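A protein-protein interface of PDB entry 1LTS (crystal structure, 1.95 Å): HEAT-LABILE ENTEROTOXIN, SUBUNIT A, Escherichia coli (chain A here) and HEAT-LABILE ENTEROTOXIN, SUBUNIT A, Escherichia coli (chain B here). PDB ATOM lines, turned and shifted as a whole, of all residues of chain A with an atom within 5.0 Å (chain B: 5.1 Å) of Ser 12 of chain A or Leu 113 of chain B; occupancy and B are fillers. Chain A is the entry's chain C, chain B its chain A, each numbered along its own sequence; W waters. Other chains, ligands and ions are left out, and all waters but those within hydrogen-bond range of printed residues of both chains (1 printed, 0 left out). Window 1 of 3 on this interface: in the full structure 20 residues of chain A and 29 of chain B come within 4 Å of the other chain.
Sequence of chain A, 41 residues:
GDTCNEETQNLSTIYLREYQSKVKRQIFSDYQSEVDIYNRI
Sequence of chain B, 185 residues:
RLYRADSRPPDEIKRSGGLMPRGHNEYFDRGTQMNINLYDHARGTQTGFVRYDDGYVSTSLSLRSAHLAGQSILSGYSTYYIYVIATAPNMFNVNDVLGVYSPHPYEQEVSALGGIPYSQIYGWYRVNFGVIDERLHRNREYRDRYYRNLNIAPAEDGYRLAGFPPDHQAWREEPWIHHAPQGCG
Among the printed residues, merely in contact across the chains: Leu 11 of chain A with Leu 161 of chain B, Ser 12 of chain A with Ile 36 of chain B, Ser 12 of chain A with Leu 113 of chain B, Ser 12 of chain A with Leu 161 of chain B, Thr 13 of chain A with Ile 36 of chain B, Tyr 15 of chain A with Phe 92 of chain B, Tyr 15 of chain A with Leu 113 of chain B, Leu 16 of chain A with Leu 113 of chain B and Leu 16 of chain A with Gly 114 of chain B.
N of Ile 36 of chain B lies close to NE2 of Gln 9 of chain A.
Of the 10 printed residues of chain A, 6 touch a printed residue of chain B. Along chain A the printed residues that touch a printed residue of chain B span positions 9 to 16. Among the printed residues, no Asp or Glu carboxylate lies within 4 Å of a Lys or Arg side-chain nitrogen of the other chain.
Of chain B, only Ile 36, Leu 113 and Leu 161 come within 4 Å of Ser 12 of chain A. Printed residues of chain B within 4 Å of Thr 13 of chain A: Ile 36. Ile 14 of chain A touches none of the printed residues of chain B. Of the printed residues of chain A, Ile 36 of chain B touches Gln 9, Ser 12 and Thr 13. Of chain A, only Ser 12 (3.98 Å), Tyr 15 (3.8 Å) and Leu 16 (3.5 Å) come within 4 Å of Leu 113 of chain B. Printed residues of chain A within 4 Å of Gly 114 of chain B: Leu 16. Of the printed residues of chain A, Leu 161 of chain B touches Leu 11 (3.8 Å) and Ser 12 (3.5 Å). The nearest residue of chain B that does not touch Ser 12 of chain A is Tyr 56 of chain B (4.7 Å). The nearest printed residue of chain A that does not touch Leu 113 of chain B is Thr 13 of chain A (5.5 Å). The nearest printed residue of chain A that does not touch Gly 114 of chain B is Ser 12 of chain A (7.2 Å).
Water W1 lies within hydrogen-bond range of the backbone carbonyl oxygen (O) of Leu 161 of chain B, the side-chain hydroxyl (OH) of Tyr 56 of chain B and the side-chain hydroxyl (OG) of Ser 12 of chain A.
The backbone carbonyl oxygen (O) of Gly 55 of chain B sits at hydrogen-bond distance from the backbone NH (N) of Gly 114 of chain B, 2.9 Å away. The backbone carbonyl oxygen (O) of Asn 90 of chain B lies within hydrogen-bond range of the backbone NH (N) of Leu 113 of chain B (2.8 Å). N of Phe 92 of chain B is in hydrogen-bond range of O of Ser 111 of chain B (2.8 Å). The backbone carbonyl oxygen (O) of Thr 8 of chain A lies within hydrogen-bond range of the side-chain hydroxyl (OG) of Ser 12 of chain A, 2.8 Å away. The backbone carbonyl oxygen (O) of Gln 9 of chain A is in hydrogen-bond range of the side-chain hydroxyl (OG1) of Thr 13 of chain A (2.9 Å).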
ATOM      1  N   GLU A   7     -18.833  25.520   3.749  1.00  0.00           N
ATOM      2  CA  GLU A   7     -17.981  24.392   3.471  1.00  0.00           C
ATOM      3  C   GLU A   7     -16.907  24.255   4.539  1.00  0.00           C
ATOM      4  O   GLU A   7     -16.683  23.148   5.016  1.00  0.00           O
ATOM      5  CB  GLU A   7     -17.307  24.564   2.145  1.00  0.00           C
ATOM      6  CG  GLU A   7     -16.836  23.285   1.522  1.00  0.00           C
ATOM      7  CD  GLU A   7     -17.911  22.380   0.920  1.00  0.00           C
ATOM      8  OE1 GLU A   7     -19.112  22.679   0.964  1.00  0.00           O
ATOM      9  OE2 GLU A   7     -17.512  21.353   0.375  1.00  0.00           O
ATOM     10  N   THR A   8     -16.247  25.350   4.940  1.00  0.00           N
ATOM     11  CA  THR A   8     -15.233  25.319   5.975  1.00  0.00           C
ATOM     12  C   THR A   8     -15.844  24.832   7.285  1.00  0.00           C
ATOM     13  O   THR A   8     -15.280  23.956   7.951  1.00  0.00           O
ATOM     14  CB  THR A   8     -14.593  26.743   6.141  1.00  0.00           C
ATOM     15  OG1 THR A   8     -13.779  26.938   4.975  1.00  0.00           O
ATOM     16  CG2 THR A   8     -13.765  26.910   7.428  1.00  0.00           C
ATOM     17  N   GLN A   9     -17.044  25.287   7.633  1.00  0.00           N
ATOM     18  CA  GLN A   9     -17.595  24.881   8.905  1.00  0.00           C
ATOM     19  C   GLN A   9     -18.028  23.435   8.909  1.00  0.00           C
ATOM     20  O   GLN A   9     -17.931  22.716   9.902  1.00  0.00           O
ATOM     21  CB  GLN A   9     -18.744  25.778   9.240  1.00  0.00           C
ATOM     22  CG  GLN A   9     -18.239  26.423  10.522  1.00  0.00           C
ATOM     23  CD  GLN A   9     -19.068  26.007  11.726  1.00  0.00           C
ATOM     24  OE1 GLN A   9     -19.987  26.732  12.105  1.00  0.00           O
ATOM     25  NE2 GLN A   9     -18.853  24.890  12.403  1.00  0.00           N
ATOM     26  N   ASN A  10     -18.412  23.027   7.717  1.00  0.00           N
ATOM     27  CA  ASN A  10     -18.869  21.700   7.452  1.00  0.00           C
ATOM     28  C   ASN A  10     -17.707  20.703   7.380  1.00  0.00           C
ATOM     29  O   ASN A  10     -17.779  19.622   7.967  1.00  0.00           O
ATOM     30  CB  ASN A  10     -19.655  21.853   6.195  1.00  0.00           C
ATOM     31  CG  ASN A  10     -19.916  20.528   5.557  1.00  0.00           C
ATOM     32  OD1 ASN A  10     -20.616  19.706   6.139  1.00  0.00           O
ATOM     33  ND2 ASN A  10     -19.340  20.263   4.385  1.00  0.00           N
ATOM     34  N   LEU A  11     -16.574  20.985   6.755  1.00  0.00           N
ATOM     35  CA  LEU A  11     -15.457  20.068   6.753  1.00  0.00           C
ATOM     36  C   LEU A  11     -14.816  20.049   8.116  1.00  0.00           C
ATOM     37  O   LEU A  11     -14.328  18.987   8.503  1.00  0.00           O
ATOM     38  CB  LEU A  11     -14.466  20.493   5.757  1.00  0.00           C
ATOM     39  CG  LEU A  11     -15.044  20.431   4.368  1.00  0.00           C
ATOM     40  CD1 LEU A  11     -14.279  21.395   3.488  1.00  0.00           C
ATOM     41  CD2 LEU A  11     -14.979  19.020   3.844  1.00  0.00           C
ATOM     42  N   SER A  12     -14.835  21.167   8.858  1.00  0.00           N
ATOM     43  CA  SER A  12     -14.361  21.238  10.239  1.00  0.00           C
ATOM     44  C   SER A  12     -15.211  20.386  11.209  1.00  0.00           C
ATOM     45  O   SER A  12     -14.665  19.603  11.996  1.00  0.00           O
ATOM     46  CB  SER A  12     -14.347  22.730  10.649  1.00  0.00           C
ATOM     47  OG  SER A  12     -13.308  23.355   9.899  1.00  0.00           O
ATOM     48  N   THR A  13     -16.544  20.492  11.205  1.00  0.00           N
ATOM     49  CA  THR A  13     -17.418  19.640  12.008  1.00  0.00           C
ATOM     50  C   THR A  13     -17.264  18.160  11.659  1.00  0.00           C
ATOM     51  O   THR A  13     -17.316  17.330  12.553  1.00  0.00           O
ATOM     52  CB  THR A  13     -18.862  20.086  11.805  1.00  0.00           C
ATOM     53  OG1 THR A  13     -18.868  21.421  12.300  1.00  0.00           O
ATOM     54  CG2 THR A  13     -19.912  19.265  12.536  1.00  0.00           C
ATOM     55  N   ILE A  14     -17.032  17.738  10.423  1.00  0.00           N
ATOM     56  CA  ILE A  14     -16.893  16.334  10.122  1.00  0.00           C
ATOM     57  C   ILE A  14     -15.581  15.875  10.696  1.00  0.00           C
ATOM     58  O   ILE A  14     -15.567  14.820  11.297  1.00  0.00           O
ATOM     59  CB  ILE A  14     -16.970  16.173   8.606  1.00  0.00           C
ATOM     60  CG1 ILE A  14     -18.423  16.334   8.205  1.00  0.00           C
ATOM     61  CG2 ILE A  14     -16.379  14.849   8.167  1.00  0.00           C
ATOM     62  CD1 ILE A  14     -18.583  16.648   6.707  1.00  0.00           C
ATOM     63  N   TYR A  15     -14.492  16.616  10.536  1.00  0.00           N
ATOM     64  CA  TYR A  15     -13.239  16.269  11.152  1.00  0.00           C
ATOM     65  C   TYR A  15     -13.485  16.192  12.674  1.00  0.00           C
ATOM     66  O   TYR A  15     -13.005  15.208  13.272  1.00  0.00           O
ATOM     67  CB  TYR A  15     -12.184  17.344  10.829  1.00  0.00           C
ATOM     68  CG  TYR A  15     -10.759  16.967  11.200  1.00  0.00           C
ATOM     69  CD1 TYR A  15     -10.285  16.944  12.507  1.00  0.00           C
ATOM     70  CD2 TYR A  15      -9.922  16.586  10.191  1.00  0.00           C
ATOM     71  CE1 TYR A  15      -8.997  16.521  12.785  1.00  0.00           C
ATOM     72  CE2 TYR A  15      -8.646  16.183  10.466  1.00  0.00           C
ATOM     73  CZ  TYR A  15      -8.192  16.147  11.756  1.00  0.00           C
ATOM     74  OH  TYR A  15      -6.906  15.702  11.957  1.00  0.00           O
ATOM     75  N   LEU A  16     -14.197  17.140  13.338  1.00  0.00           N
ATOM     76  CA  LEU A  16     -14.463  17.047  14.776  1.00  0.00           C
ATOM     77  C   LEU A  16     -15.298  15.798  15.162  1.00  0.00           C
ATOM     78  O   LEU A  16     -14.903  15.077  16.080  1.00  0.00           O
ATOM     79  CB  LEU A  16     -15.209  18.300  15.339  1.00  0.00           C
ATOM     80  CG  LEU A  16     -15.480  18.274  16.871  1.00  0.00           C
ATOM     81  CD1 LEU A  16     -14.177  18.084  17.656  1.00  0.00           C
ATOM     82  CD2 LEU A  16     -16.162  19.518  17.261  1.00  0.00           C
ATOM     83  N   ILE B  36     -16.538  27.150  13.563  1.00  0.00           N
ATOM     84  CA  ILE B  36     -15.192  26.599  13.688  1.00  0.00           C
ATOM     85  C   ILE B  36     -14.444  27.131  12.478  1.00  0.00           C
ATOM     86  O   ILE B  36     -14.848  26.856  11.337  1.00  0.00           O
ATOM     87  CB  ILE B  36     -15.173  25.040  13.659  1.00  0.00           C
ATOM     88  CG1 ILE B  36     -16.093  24.443  14.726  1.00  0.00           C
ATOM     89  CG2 ILE B  36     -13.748  24.578  13.918  1.00  0.00           C
ATOM     90  CD1 ILE B  36     -16.296  22.923  14.653  1.00  0.00           C
ATOM     91  N   GLY B  55     -14.027  27.942  17.656  1.00  0.00           N
ATOM     92  CA  GLY B  55     -13.964  26.489  17.721  1.00  0.00           C
ATOM     93  C   GLY B  55     -12.638  25.821  17.957  1.00  0.00           C
ATOM     94  O   GLY B  55     -12.545  24.599  17.769  1.00  0.00           O
ATOM     95  N   TYR B  56     -11.621  26.557  18.390  1.00  0.00           N
ATOM     96  CA  TYR B  56     -10.331  25.963  18.649  1.00  0.00           C
ATOM     97  C   TYR B  56      -9.789  26.422  20.001  1.00  0.00           C
ATOM     98  O   TYR B  56     -10.180  27.510  20.458  1.00  0.00           O
ATOM     99  CB  TYR B  56      -9.364  26.370  17.593  1.00  0.00           C
ATOM    100  CG  TYR B  56      -9.470  25.778  16.206  1.00  0.00           C
ATOM    101  CD1 TYR B  56     -10.388  26.234  15.275  1.00  0.00           C
ATOM    102  CD2 TYR B  56      -8.565  24.796  15.887  1.00  0.00           C
ATOM    103  CE1 TYR B  56     -10.384  25.670  14.011  1.00  0.00           C
ATOM    104  CE2 TYR B  56      -8.553  24.249  14.615  1.00  0.00           C
ATOM    105  CZ  TYR B  56      -9.471  24.692  13.695  1.00  0.00           C
ATOM    106  OH  TYR B  56      -9.454  24.119  12.440  1.00  0.00           O
ATOM    107  N   ASN B  90      -6.249  15.886  16.619  1.00  0.00           N
ATOM    108  CA  ASN B  90      -7.163  17.036  16.665  1.00  0.00           C
ATOM    109  C   ASN B  90      -6.381  18.376  16.754  1.00  0.00           C
ATOM    110  O   ASN B  90      -6.968  19.462  16.774  1.00  0.00           O
ATOM    111  CB  ASN B  90      -8.110  16.947  17.883  1.00  0.00           C
ATOM    112  CG  ASN B  90      -7.474  16.872  19.274  1.00  0.00           C
ATOM    113  OD1 ASN B  90      -6.306  16.476  19.432  1.00  0.00           O
ATOM    114  ND2 ASN B  90      -8.229  17.186  20.311  1.00  0.00           N
ATOM    115  N   MET B  91      -5.053  18.333  16.865  1.00  0.00           N
ATOM    116  CA  MET B  91      -4.224  19.502  17.027  1.00  0.00           C
ATOM    117  C   MET B  91      -3.581  19.828  15.667  1.00  0.00           C
ATOM    118  O   MET B  91      -3.025  18.969  14.945  1.00  0.00           O
ATOM    119  CB  MET B  91      -3.052  19.289  18.024  1.00  0.00           C
ATOM    120  CG  MET B  91      -3.186  18.843  19.489  1.00  0.00           C
ATOM    121  SD  MET B  91      -4.316  19.800  20.513  1.00  0.00           S
ATOM    122  CE  MET B  91      -3.500  21.348  20.647  1.00  0.00           C
ATOM    123  N   PHE B  92      -3.598  21.134  15.365  1.00  0.00           N
ATOM    124  CA  PHE B  92      -2.934  21.689  14.190  1.00  0.00           C
ATOM    125  C   PHE B  92      -1.888  22.769  14.537  1.00  0.00           C
ATOM    126  O   PHE B  92      -2.134  23.691  15.330  1.00  0.00           O
ATOM    127  CB  PHE B  92      -3.989  22.269  13.300  1.00  0.00           C
ATOM    128  CG  PHE B  92      -4.960  21.274  12.684  1.00  0.00           C
ATOM    129  CD1 PHE B  92      -4.655  20.660  11.476  1.00  0.00           C
ATOM    130  CD2 PHE B  92      -6.164  21.022  13.311  1.00  0.00           C
ATOM    131  CE1 PHE B  92      -5.574  19.794  10.894  1.00  0.00           C
ATOM    132  CE2 PHE B  92      -7.057  20.153  12.707  1.00  0.00           C
ATOM    133  CZ  PHE B  92      -6.773  19.540  11.506  1.00  0.00           C
ATOM    134  N   SER B 111      -3.200  24.538  17.855  1.00  0.00           N
ATOM    135  CA  SER B 111      -4.580  24.670  18.233  1.00  0.00           C
ATOM    136  C   SER B 111      -5.374  23.388  18.079  1.00  0.00           C
ATOM    137  O   SER B 111      -5.225  22.641  17.104  1.00  0.00           O
ATOM    138  CB  SER B 111      -5.163  25.778  17.393  1.00  0.00           C
ATOM    139  OG  SER B 111      -4.916  26.963  18.145  1.00  0.00           O
ATOM    140  N   ALA B 112      -6.225  23.127  19.057  1.00  0.00           N
ATOM    141  CA  ALA B 112      -7.006  21.905  19.071  1.00  0.00           C
ATOM    142  C   ALA B 112      -8.415  22.184  18.587  1.00  0.00           C
ATOM    143  O   ALA B 112      -9.135  23.042  19.145  1.00  0.00           O
ATOM    144  CB  ALA B 112      -7.067  21.356  20.479  1.00  0.00           C
ATOM    145  N   LEU B 113      -8.759  21.502  17.483  1.00  0.00           N
ATOM    146  CA  LEU B 113     -10.073  21.593  16.890  1.00  0.00           C
ATOM    147  C   LEU B 113     -11.142  21.002  17.803  1.00  0.00           C
ATOM    148  O   LEU B 113     -11.116  19.819  18.092  1.00  0.00           O
ATOM    149  CB  LEU B 113      -9.995  20.887  15.508  1.00  0.00           C
ATOM    150  CG  LEU B 113     -11.230  20.562  14.574  1.00  0.00           C
ATOM    151  CD1 LEU B 113     -12.428  21.459  14.711  1.00  0.00           C
ATOM    152  CD2 LEU B 113     -10.728  20.709  13.171  1.00  0.00           C
ATOM    153  N   GLY B 114     -12.066  21.832  18.279  1.00  0.00           N
ATOM    154  CA  GLY B 114     -13.174  21.444  19.117  1.00  0.00           C
ATOM    155  C   GLY B 114     -12.837  21.374  20.577  1.00  0.00           C
ATOM    156  O   GLY B 114     -13.707  21.028  21.374  1.00  0.00           O
ATOM    157  N   GLY B 115     -11.647  21.737  21.007  1.00  0.00           N
ATOM    158  CA  GLY B 115     -11.326  21.646  22.414  1.00  0.00           C
ATOM    159  C   GLY B 115     -10.431  20.450  22.660  1.00  0.00           C
ATOM    160  O   GLY B 115     -10.077  19.709  21.726  1.00  0.00           O
ATOM    161  N   LEU B 161      -8.817  23.191   5.897  1.00  0.00           N
ATOM    162  CA  LEU B 161      -9.465  23.707   7.091  1.00  0.00           C
ATOM    163  C   LEU B 161      -9.028  25.108   7.530  1.00  0.00           C
ATOM    164  O   LEU B 161      -9.546  25.628   8.529  1.00  0.00           O
ATOM    165  CB  LEU B 161      -9.241  22.716   8.280  1.00  0.00           C
ATOM    166  CG  LEU B 161      -9.792  21.279   8.204  1.00  0.00           C
ATOM    167  CD1 LEU B 161      -9.537  20.544   9.494  1.00  0.00           C
ATOM    168  CD2 LEU B 161     -11.295  21.331   7.960  1.00  0.00           C
HETATM  169  O   HOH W   1     -11.311  25.306  10.669  1.00  0.00           O
